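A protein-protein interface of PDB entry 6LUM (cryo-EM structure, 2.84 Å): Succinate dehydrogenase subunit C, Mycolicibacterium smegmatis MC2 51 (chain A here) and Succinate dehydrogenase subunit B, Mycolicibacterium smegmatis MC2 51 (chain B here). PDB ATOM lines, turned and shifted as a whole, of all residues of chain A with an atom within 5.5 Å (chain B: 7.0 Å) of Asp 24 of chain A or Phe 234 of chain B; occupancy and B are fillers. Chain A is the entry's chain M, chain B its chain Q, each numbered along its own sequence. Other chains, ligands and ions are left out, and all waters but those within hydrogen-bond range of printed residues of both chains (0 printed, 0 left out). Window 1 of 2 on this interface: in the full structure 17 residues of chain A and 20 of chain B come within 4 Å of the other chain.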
ATOM      1  N   TYR A  21       4.175   2.143  -4.556  1.00  0.00           N
ATOM      2  CA  TYR A  21       3.523   1.663  -3.345  1.00  0.00           C
ATOM      3  C   TYR A  21       4.218   0.441  -2.770  1.00  0.00           C
ATOM      4  O   TYR A  21       4.228   0.270  -1.549  1.00  0.00           O
ATOM      5  CB  TYR A  21       2.053   1.347  -3.582  1.00  0.00           C
ATOM      6  CG  TYR A  21       1.432   0.695  -2.371  1.00  0.00           C
ATOM      7  CD1 TYR A  21       1.111   1.431  -1.248  1.00  0.00           C
ATOM      8  CD2 TYR A  21       1.216  -0.664  -2.333  1.00  0.00           C
ATOM      9  CE1 TYR A  21       0.577   0.831  -0.142  1.00  0.00           C
ATOM     10  CE2 TYR A  21       0.688  -1.260  -1.232  1.00  0.00           C
ATOM     11  CZ  TYR A  21       0.369  -0.514  -0.144  1.00  0.00           C
ATOM     12  OH  TYR A  21      -0.169  -1.143   0.943  1.00  0.00           O
ATOM     13  N   ARG A  22       4.806  -0.412  -3.600  1.00  0.00           N
ATOM     14  CA  ARG A  22       5.560  -1.555  -3.096  1.00  0.00           C
ATOM     15  C   ARG A  22       4.659  -2.476  -2.274  1.00  0.00           C
ATOM     16  O   ARG A  22       4.815  -2.632  -1.066  1.00  0.00           O
ATOM     17  CB  ARG A  22       6.763  -1.074  -2.277  1.00  0.00           C
ATOM     18  CG  ARG A  22       7.738  -2.134  -1.847  1.00  0.00           C
ATOM     19  CD  ARG A  22       8.989  -1.497  -1.275  1.00  0.00           C
ATOM     20  NE  ARG A  22       9.801  -0.865  -2.312  1.00  0.00           N
ATOM     21  CZ  ARG A  22       9.801   0.437  -2.578  1.00  0.00           C
ATOM     22  NH1 ARG A  22      10.572   0.918  -3.541  1.00  0.00           N
ATOM     23  NH2 ARG A  22       9.031   1.258  -1.881  1.00  0.00           N
ATOM     24  N   GLY A  23       3.695  -3.075  -2.956  1.00  0.00           N
ATOM     25  CA  GLY A  23       2.683  -3.907  -2.329  1.00  0.00           C
ATOM     26  C   GLY A  23       2.847  -5.378  -2.644  1.00  0.00           C
ATOM     27  O   GLY A  23       3.954  -5.924  -2.601  1.00  0.00           O
ATOM     28  N   ASP A  24       1.737  -6.021  -2.963  1.00  0.00           N
ATOM     29  CA  ASP A  24       1.639  -7.464  -3.098  1.00  0.00           C
ATOM     30  C   ASP A  24       2.077  -7.911  -4.493  1.00  0.00           C
ATOM     31  O   ASP A  24       1.944  -7.159  -5.459  1.00  0.00           O
ATOM     32  CB  ASP A  24       0.205  -7.904  -2.860  1.00  0.00           C
ATOM     33  CG  ASP A  24       0.112  -9.170  -2.060  1.00  0.00           C
ATOM     34  OD1 ASP A  24       1.132  -9.592  -1.492  1.00  0.00           O
ATOM     35  OD2 ASP A  24      -0.982  -9.754  -1.997  1.00  0.00           O
ATOM     36  N   PRO A  25       2.613  -9.128  -4.627  1.00  0.00           N
ATOM     37  CA  PRO A  25       2.843  -9.680  -5.968  1.00  0.00           C
ATOM     38  C   PRO A  25       1.590  -9.776  -6.816  1.00  0.00           C
ATOM     39  O   PRO A  25       1.692  -9.781  -8.049  1.00  0.00           O
ATOM     40  CB  PRO A  25       3.428 -11.068  -5.678  1.00  0.00           C
ATOM     41  CG  PRO A  25       3.220 -11.294  -4.225  1.00  0.00           C
ATOM     42  CD  PRO A  25       3.256  -9.958  -3.604  1.00  0.00           C
ATOM     43  N   GLY A  26       0.415  -9.863  -6.202  1.00  0.00           N
ATOM     44  CA  GLY A  26      -0.812  -9.809  -6.970  1.00  0.00           C
ATOM     45  C   GLY A  26      -0.976  -8.504  -7.712  1.00  0.00           C
ATOM     46  O   GLY A  26      -1.582  -8.469  -8.782  1.00  0.00           O
ATOM     47  N   MET A  27      -0.409  -7.424  -7.182  1.00  0.00           N
ATOM     48  CA  MET A  27      -0.488  -6.128  -7.845  1.00  0.00           C
ATOM     49  C   MET A  27       0.313  -6.116  -9.138  1.00  0.00           C
ATOM     50  O   MET A  27      -0.145  -5.599 -10.164  1.00  0.00           O
ATOM     51  CB  MET A  27       0.004  -5.051  -6.889  1.00  0.00           C
ATOM     52  CG  MET A  27      -0.007  -3.656  -7.425  1.00  0.00           C
ATOM     53  SD  MET A  27       1.147  -2.652  -6.494  1.00  0.00           S
ATOM     54  CE  MET A  27       0.617  -1.036  -6.981  1.00  0.00           C
ATOM     55  N   TRP A  28       1.506  -6.698  -9.113  1.00  0.00           N
ATOM     56  CA  TRP A  28       2.321  -6.757 -10.313  1.00  0.00           C
ATOM     57  C   TRP A  28       1.752  -7.741 -11.319  1.00  0.00           C
ATOM     58  O   TRP A  28       1.796  -7.494 -12.528  1.00  0.00           O
ATOM     59  CB  TRP A  28       3.744  -7.112  -9.927  1.00  0.00           C
ATOM     60  CG  TRP A  28       4.283  -6.142  -8.944  1.00  0.00           C
ATOM     61  CD1 TRP A  28       4.683  -6.400  -7.675  1.00  0.00           C
ATOM     62  CD2 TRP A  28       4.464  -4.743  -9.145  1.00  0.00           C
ATOM     63  NE1 TRP A  28       5.110  -5.250  -7.072  1.00  0.00           N
ATOM     64  CE2 TRP A  28       4.985  -4.216  -7.960  1.00  0.00           C
ATOM     65  CE3 TRP A  28       4.240  -3.884 -10.220  1.00  0.00           C
ATOM     66  CZ2 TRP A  28       5.283  -2.873  -7.815  1.00  0.00           C
ATOM     67  CZ3 TRP A  28       4.534  -2.560 -10.074  1.00  0.00           C
ATOM     68  CH2 TRP A  28       5.048  -2.063  -8.886  1.00  0.00           C
ATOM     69  N   ARG A  93      -5.492 -18.289 -13.474  1.00  0.00           N
ATOM     70  CA  ARG A  93      -5.371 -18.014 -12.043  1.00  0.00           C
ATOM     71  C   ARG A  93      -6.542 -17.184 -11.536  1.00  0.00           C
ATOM     72  O   ARG A  93      -7.123 -17.482 -10.491  1.00  0.00           O
ATOM     73  CB  ARG A  93      -4.063 -17.295 -11.759  1.00  0.00           C
ATOM     74  CG  ARG A  93      -3.830 -17.023 -10.313  1.00  0.00           C
ATOM     75  CD  ARG A  93      -2.565 -16.233 -10.117  1.00  0.00           C
ATOM     76  NE  ARG A  93      -2.814 -14.801 -10.158  1.00  0.00           N
ATOM     77  CZ  ARG A  93      -2.972 -14.054  -9.078  1.00  0.00           C
ATOM     78  NH1 ARG A  93      -2.884 -14.610  -7.893  1.00  0.00           N
ATOM     79  NH2 ARG A  93      -3.204 -12.757  -9.175  1.00  0.00           N
ATOM     80  N   ILE A  97      -9.404 -18.171  -8.784  1.00  0.00           N
ATOM     81  CA  ILE A  97      -9.667 -17.342  -7.611  1.00  0.00           C
ATOM     82  C   ILE A  97     -11.147 -17.026  -7.498  1.00  0.00           C
ATOM     83  O   ILE A  97     -11.731 -17.093  -6.413  1.00  0.00           O
ATOM     84  CB  ILE A  97      -8.833 -16.055  -7.673  1.00  0.00           C
ATOM     85  CG1 ILE A  97      -7.406 -16.334  -7.240  1.00  0.00           C
ATOM     86  CG2 ILE A  97      -9.447 -15.007  -6.811  1.00  0.00           C
ATOM     87  CD1 ILE A  97      -6.574 -15.122  -7.188  1.00  0.00           C
ATOM     88  N   PRO A 104      -8.658 -17.543  -3.078  1.00  0.00           N
ATOM     89  CA  PRO A 104      -7.982 -16.427  -2.408  1.00  0.00           C
ATOM     90  C   PRO A 104      -7.019 -16.855  -1.318  1.00  0.00           C
ATOM     91  O   PRO A 104      -6.113 -16.104  -0.949  1.00  0.00           O
ATOM     92  CB  PRO A 104      -9.149 -15.625  -1.834  1.00  0.00           C
ATOM     93  CG  PRO A 104     -10.239 -15.879  -2.741  1.00  0.00           C
ATOM     94  CD  PRO A 104     -10.108 -17.308  -3.146  1.00  0.00           C
ATOM     95  N   GLN A 107      -3.820 -18.186  -3.557  1.00  0.00           N
ATOM     96  CA  GLN A 107      -3.063 -17.191  -4.298  1.00  0.00           C
ATOM     97  C   GLN A 107      -1.615 -17.192  -3.823  1.00  0.00           C
ATOM     98  O   GLN A 107      -1.311 -17.619  -2.706  1.00  0.00           O
ATOM     99  CB  GLN A 107      -3.706 -15.820  -4.095  1.00  0.00           C
ATOM    100  CG  GLN A 107      -3.000 -14.655  -4.724  1.00  0.00           C
ATOM    101  CD  GLN A 107      -2.223 -13.838  -3.727  1.00  0.00           C
ATOM    102  OE1 GLN A 107      -2.388 -14.001  -2.525  1.00  0.00           O
ATOM    103  NE2 GLN A 107      -1.385 -12.937  -4.218  1.00  0.00           N
ATOM    104  N   ARG A 108      -0.713 -16.762  -4.701  1.00  0.00           N
ATOM    105  CA  ARG A 108       0.718 -16.661  -4.423  1.00  0.00           C
ATOM    106  C   ARG A 108       1.365 -18.036  -4.379  1.00  0.00           C
ATOM    107  O   ARG A 108       2.592 -18.150  -4.318  1.00  0.00           O
ATOM    108  CB  ARG A 108       0.986 -15.912  -3.119  1.00  0.00           C
ATOM    109  CG  ARG A 108       2.325 -15.224  -3.074  1.00  0.00           C
ATOM    110  CD  ARG A 108       2.579 -14.633  -1.708  1.00  0.00           C
ATOM    111  NE  ARG A 108       1.517 -13.722  -1.304  1.00  0.00           N
ATOM    112  CZ  ARG A 108       1.633 -12.841  -0.318  1.00  0.00           C
ATOM    113  NH1 ARG A 108       2.763 -12.753   0.363  1.00  0.00           N
ATOM    114  NH2 ARG A 108       0.618 -12.046  -0.016  1.00  0.00           N
ATOM    115  N   VAL B  92       4.588   0.684   2.380  1.00  0.00           N
ATOM    116  CA  VAL B  92       3.373  -0.060   2.684  1.00  0.00           C
ATOM    117  C   VAL B  92       2.568   0.653   3.758  1.00  0.00           C
ATOM    118  O   VAL B  92       3.121   1.320   4.629  1.00  0.00           O
ATOM    119  CB  VAL B  92       3.715  -1.497   3.124  1.00  0.00           C
ATOM    120  CG1 VAL B  92       4.126  -2.311   1.949  1.00  0.00           C
ATOM    121  CG2 VAL B  92       4.834  -1.478   4.124  1.00  0.00           C
ATOM    122  N   SER B 183      -4.902   1.200  -0.147  1.00  0.00           N
ATOM    123  CA  SER B 183      -3.928   0.446  -0.921  1.00  0.00           C
ATOM    124  C   SER B 183      -4.560  -0.202  -2.138  1.00  0.00           C
ATOM    125  O   SER B 183      -3.904  -0.998  -2.804  1.00  0.00           O
ATOM    126  CB  SER B 183      -3.251  -0.609  -0.061  1.00  0.00           C
ATOM    127  OG  SER B 183      -4.212  -1.449   0.513  1.00  0.00           O
ATOM    128  N   ARG B 231     -10.278  -5.827  -8.985  1.00  0.00           N
ATOM    129  CA  ARG B 231      -9.402  -6.470  -9.946  1.00  0.00           C
ATOM    130  C   ARG B 231      -8.596  -7.594  -9.336  1.00  0.00           C
ATOM    131  O   ARG B 231      -7.575  -7.986  -9.901  1.00  0.00           O
ATOM    132  CB  ARG B 231      -8.471  -5.444 -10.577  1.00  0.00           C
ATOM    133  CG  ARG B 231      -9.173  -4.452 -11.477  1.00  0.00           C
ATOM    134  CD  ARG B 231      -9.400  -4.998 -12.866  1.00  0.00           C
ATOM    135  NE  ARG B 231     -10.616  -5.790 -12.961  1.00  0.00           N
ATOM    136  CZ  ARG B 231     -11.834  -5.279 -13.038  1.00  0.00           C
ATOM    137  NH1 ARG B 231     -12.004  -3.971 -13.032  1.00  0.00           N
ATOM    138  NH2 ARG B 231     -12.885  -6.074 -13.117  1.00  0.00           N
ATOM    139  N   THR B 232      -9.034  -8.115  -8.195  1.00  0.00           N
ATOM    140  CA  THR B 232      -8.415  -9.258  -7.532  1.00  0.00           C
ATOM    141  C   THR B 232      -6.930  -9.012  -7.297  1.00  0.00           C
ATOM    142  O   THR B 232      -6.079  -9.870  -7.520  1.00  0.00           O
ATOM    143  CB  THR B 232      -8.656 -10.542  -8.312  1.00  0.00           C
ATOM    144  OG1 THR B 232     -10.056 -10.673  -8.553  1.00  0.00           O
ATOM    145  CG2 THR B 232      -8.267 -11.730  -7.488  1.00  0.00           C
ATOM    146  N   THR B 233      -6.612  -7.808  -6.872  1.00  0.00           N
ATOM    147  CA  THR B 233      -5.363  -7.566  -6.186  1.00  0.00           C
ATOM    148  C   THR B 233      -5.598  -7.792  -4.698  1.00  0.00           C
ATOM    149  O   THR B 233      -6.699  -7.525  -4.166  1.00  0.00           O
ATOM    150  CB  THR B 233      -4.866  -6.146  -6.430  1.00  0.00           C
ATOM    151  OG1 THR B 233      -4.996  -5.812  -7.810  1.00  0.00           O
ATOM    152  CG2 THR B 233      -3.452  -6.048  -6.055  1.00  0.00           C
ATOM    153  N   PHE B 234      -4.564  -8.303  -4.032  1.00  0.00           N
ATOM    154  CA  PHE B 234      -4.619  -8.661  -2.624  1.00  0.00           C
ATOM    155  C   PHE B 234      -3.853  -7.666  -1.765  1.00  0.00           C
ATOM    156  O   PHE B 234      -3.361  -8.003  -0.686  1.00  0.00           O
ATOM    157  CB  PHE B 234      -4.092 -10.077  -2.418  1.00  0.00           C
ATOM    158  CG  PHE B 234      -4.923 -11.132  -3.080  1.00  0.00           C
ATOM    159  CD1 PHE B 234      -4.886 -11.307  -4.442  1.00  0.00           C
ATOM    160  CD2 PHE B 234      -5.742 -11.949  -2.336  1.00  0.00           C
ATOM    161  CE1 PHE B 234      -5.651 -12.263  -5.045  1.00  0.00           C
ATOM    162  CE2 PHE B 234      -6.504 -12.909  -2.940  1.00  0.00           C
ATOM    163  CZ  PHE B 234      -6.459 -13.064  -4.295  1.00  0.00           C
ATOM    164  N   ASN B 235      -3.748  -6.430  -2.244  1.00  0.00           N
ATOM    165  CA  ASN B 235      -3.158  -5.363  -1.453  1.00  0.00           C
ATOM    166  C   ASN B 235      -3.914  -5.164  -0.150  1.00  0.00           C
ATOM    167  O   ASN B 235      -3.308  -4.960   0.906  1.00  0.00           O
ATOM    168  CB  ASN B 235      -3.150  -4.077  -2.264  1.00  0.00           C
ATOM    169  CG  ASN B 235      -1.881  -3.883  -3.031  1.00  0.00           C
ATOM    170  OD1 ASN B 235      -1.042  -4.763  -3.084  1.00  0.00           O
ATOM    171  ND2 ASN B 235      -1.726  -2.721  -3.624  1.00  0.00           N
ATOM    172  N   CYS B 236      -5.244  -5.222  -0.204  1.00  0.00           N
ATOM    173  CA  CYS B 236      -6.051  -5.089   1.002  1.00  0.00           C
ATOM    174  C   CYS B 236      -5.711  -6.172   2.010  1.00  0.00           C
ATOM    175  O   CYS B 236      -5.503  -5.895   3.199  1.00  0.00           O
ATOM    176  CB  CYS B 236      -7.524  -5.157   0.633  1.00  0.00           C
ATOM    177  SG  CYS B 236      -7.939  -6.566  -0.367  1.00  0.00           S
ATOM    178  N   THR B 237      -5.649  -7.419   1.544  1.00  0.00           N
ATOM    179  CA  THR B 237      -5.391  -8.543   2.431  1.00  0.00           C
ATOM    180  C   THR B 237      -4.003  -8.461   3.037  1.00  0.00           C
ATOM    181  O   THR B 237      -3.807  -8.823   4.200  1.00  0.00           O
ATOM    182  CB  THR B 237      -5.560  -9.856   1.677  1.00  0.00           C
ATOM    183  OG1 THR B 237      -6.850  -9.898   1.064  1.00  0.00           O
ATOM    184  CG2 THR B 237      -5.435 -11.010   2.613  1.00  0.00           C
ATOM    185  N   GLU B 238      -3.022  -7.993   2.273  1.00  0.00           N
ATOM    186  CA  GLU B 238      -1.689  -7.896   2.843  1.00  0.00           C
ATOM    187  C   GLU B 238      -1.520  -6.667   3.719  1.00  0.00           C
ATOM    188  O   GLU B 238      -0.571  -6.616   4.506  1.00  0.00           O
ATOM    189  CB  GLU B 238      -0.634  -7.918   1.736  1.00  0.00           C
ATOM    190  CG  GLU B 238      -0.656  -6.742   0.791  1.00  0.00           C
ATOM    191  CD  GLU B 238       0.382  -5.685   1.112  1.00  0.00           C
ATOM    192  OE1 GLU B 238       1.402  -6.029   1.739  1.00  0.00           O
ATOM    193  OE2 GLU B 238       0.179  -4.511   0.738  1.00  0.00           O
ATOM    194  N   ALA B 239      -2.419  -5.686   3.625  1.00  0.00           N
ATOM    195  CA  ALA B 239      -2.287  -4.473   4.418  1.00  0.00           C
ATOM    196  C   ALA B 239      -3.094  -4.469   5.704  1.00  0.00           C
ATOM    197  O   ALA B 239      -2.751  -3.705   6.609  1.00  0.00           O
ATOM    198  CB  ALA B 239      -2.689  -3.255   3.591  1.00  0.00           C
ATOM    199  N   GLN B 245      -8.745 -11.119   5.734  1.00  0.00           N
ATOM    200  CA  GLN B 245      -9.000 -11.805   4.470  1.00  0.00           C
ATOM    201  C   GLN B 245     -10.026 -11.024   3.655  1.00  0.00           C
ATOM    202  O   GLN B 245     -11.117 -11.496   3.319  1.00  0.00           O
ATOM    203  CB  GLN B 245      -9.443 -13.250   4.700  1.00  0.00           C
ATOM    204  CG  GLN B 245      -8.606 -13.994   5.717  1.00  0.00           C
ATOM    205  CD  GLN B 245      -7.192 -14.227   5.251  1.00  0.00           C
ATOM    206  OE1 GLN B 245      -6.253 -14.186   6.041  1.00  0.00           O
ATOM    207  NE2 GLN B 245      -7.028 -14.480   3.962  1.00  0.00           N
ATOM    208  N   VAL B 246      -9.643  -9.786   3.365  1.00  0.00           N
ATOM    209  CA  VAL B 246     -10.535  -8.836   2.729  1.00  0.00           C
ATOM    210  C   VAL B 246     -10.923  -9.321   1.345  1.00  0.00           C
ATOM    211  O   VAL B 246     -12.059  -9.120   0.899  1.00  0.00           O
ATOM    212  CB  VAL B 246      -9.849  -7.461   2.704  1.00  0.00           C
ATOM    213  CG1 VAL B 246     -10.823  -6.389   2.391  1.00  0.00           C
ATOM    214  CG2 VAL B 246      -9.172  -7.191   4.024  1.00  0.00           C
ATOM    215  N   THR B 247     -10.018 -10.014   0.663  1.00  0.00           N
ATOM    216  CA  THR B 247     -10.338 -10.507  -0.667  1.00  0.00           C
ATOM    217  C   THR B 247     -11.233 -11.736  -0.618  1.00  0.00           C
ATOM    218  O   THR B 247     -12.076 -11.907  -1.499  1.00  0.00           O
ATOM    219  CB  THR B 247      -9.058 -10.804  -1.431  1.00  0.00           C
ATOM    220  OG1 THR B 247      -8.108  -9.777  -1.150  1.00  0.00           O
ATOM    221  CG2 THR B 247      -9.336 -10.788  -2.913  1.00  0.00           C
ATOM    222  N   GLN B 248     -11.085 -12.593   0.393  1.00  0.00           N
ATOM    223  CA  GLN B 248     -12.067 -13.651   0.599  1.00  0.00           C
ATOM    224  C   GLN B 248     -13.456 -13.077   0.818  1.00  0.00           C
ATOM    225  O   GLN B 248     -14.438 -13.585   0.269  1.00  0.00           O
ATOM    226  CB  GLN B 248     -11.684 -14.521   1.786  1.00  0.00           C
ATOM    227  CG  GLN B 248     -10.668 -15.580   1.490  1.00  0.00           C
ATOM    228  CD  GLN B 248     -10.633 -16.646   2.557  1.00  0.00           C
ATOM    229  OE1 GLN B 248     -11.407 -16.609   3.506  1.00  0.00           O
ATOM    230  NE2 GLN B 248      -9.729 -17.599   2.411  1.00  0.00           N
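The side-chain carboxylate of Glu 238 of chain B lies within hydrogen-bond range of the side-chain hydroxyl of Tyr 21 of chain A, 3.4 Å away. The backbone NH (N) of Asp 24 of chain A lies within hydrogen-bond range of the side-chain amide oxygen (OD1) of Asn 235 of chain B (3.1 Å). The side-chain carboxylate (OD2) of Asp 24 of chain A lies close to the backbone carbonyl oxygen (O) of Phe 234 of chain B (3.2 Å).
The guanidinium group (NH2) of Arg 108 of chain A lies within salt-bridge range of the side-chain carboxylate (OD1) of Asp 24 of chain A, 2.9 Å away. The side-chain amide nitrogen (ND2) of Asn 235 of chain B is in hydrogen-bond range of the backbone carbonyl oxygen (O) of Ser 183 of chain B (2.9 Å).
Among the printed residues, pairs that only touch across the chains: Arg 22 of chain A with Val 92 of chain B, Tyr 21 of chain A with Ser 183 of chain B, Met 27 of chain A with Thr 233 of chain B, Ile 97 of chain A with Thr 232 of chain B, Ile 97 of chain A with Phe 234 of chain B, Gln 107 of chain A with Phe 234 of chain B, Pro 104 of chain A with Gln 248 of chain B, Tyr 21 of chain A with Asn 235 of chain B, Pro 104 of chain A with Phe 234 of chain B, Asp 24 of chain A with Glu 238 of chain B, Gly 26 of chain A with Thr 233 of chain B, Gly 23 of chain A with Asn 235 of chain B, Met 27 of chain A with Asn 235 of chain B and Tyr 21 of chain A with Val 92 of chain B.
Of chain B, only Phe 234 (3.2 Å), Asn 235 (3.1 Å) and Glu 238 (3.8 Å) come within 4 Å of Asp 24 of chain A. Of chain A, only Asp 24, Ile 97, Pro 104 and Gln 107 come within 4 Å of Phe 234 of chain B. Of the printed residues of chain A, Thr 232 of chain B touches Ile 97. Of the printed residues of chain A, Ser 183 of chain B touches Tyr 21. Of the printed residues of chain A, Thr 233 of chain B touches Gly 26 and Met 27. Of the printed residues of chain B, Arg 22 of chain A touches Val 92. Val 246 of chain B touches none of the printed residues of chain A. Ala 239 of chain B touches none of the printed residues of chain A. The nearest residue of chain B that does not touch Asp 24 of chain A is Thr 233 of chain B (5.2 Å). The nearest residue of chain A that does not touch Phe 234 of chain B is Arg 93 of chain A (4.6 Å). The nearest printed residue of chain A that does not touch Ser 183 of chain B is Met 27 of chain A (6.2 Å).
Of the 13 printed residues of chain A, 9 touch a printed residue of chain B. Printed residues of chain A that touch a printed residue of chain B: Tyr 21, Arg 22, Gly 23, Asp 24, Gly 26, Met 27, Ile 97, Pro 104 and Gln 107. Hydrophobic or aromatic side chains of chain A that line the printed part of chain B: Tyr 21, Met 27, Ile 97 and Pro 104. Hydrophobic or aromatic side chains of chain B within 4 Å of the printed part of chain A: Val 92 and Phe 234. Among the printed residues, 17 pairs touch across the chains. Among the printed residues, no Asp or Glu carboxylate lies within 4 Å of a Lys or Arg side-chain nitrogen of the other chain.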
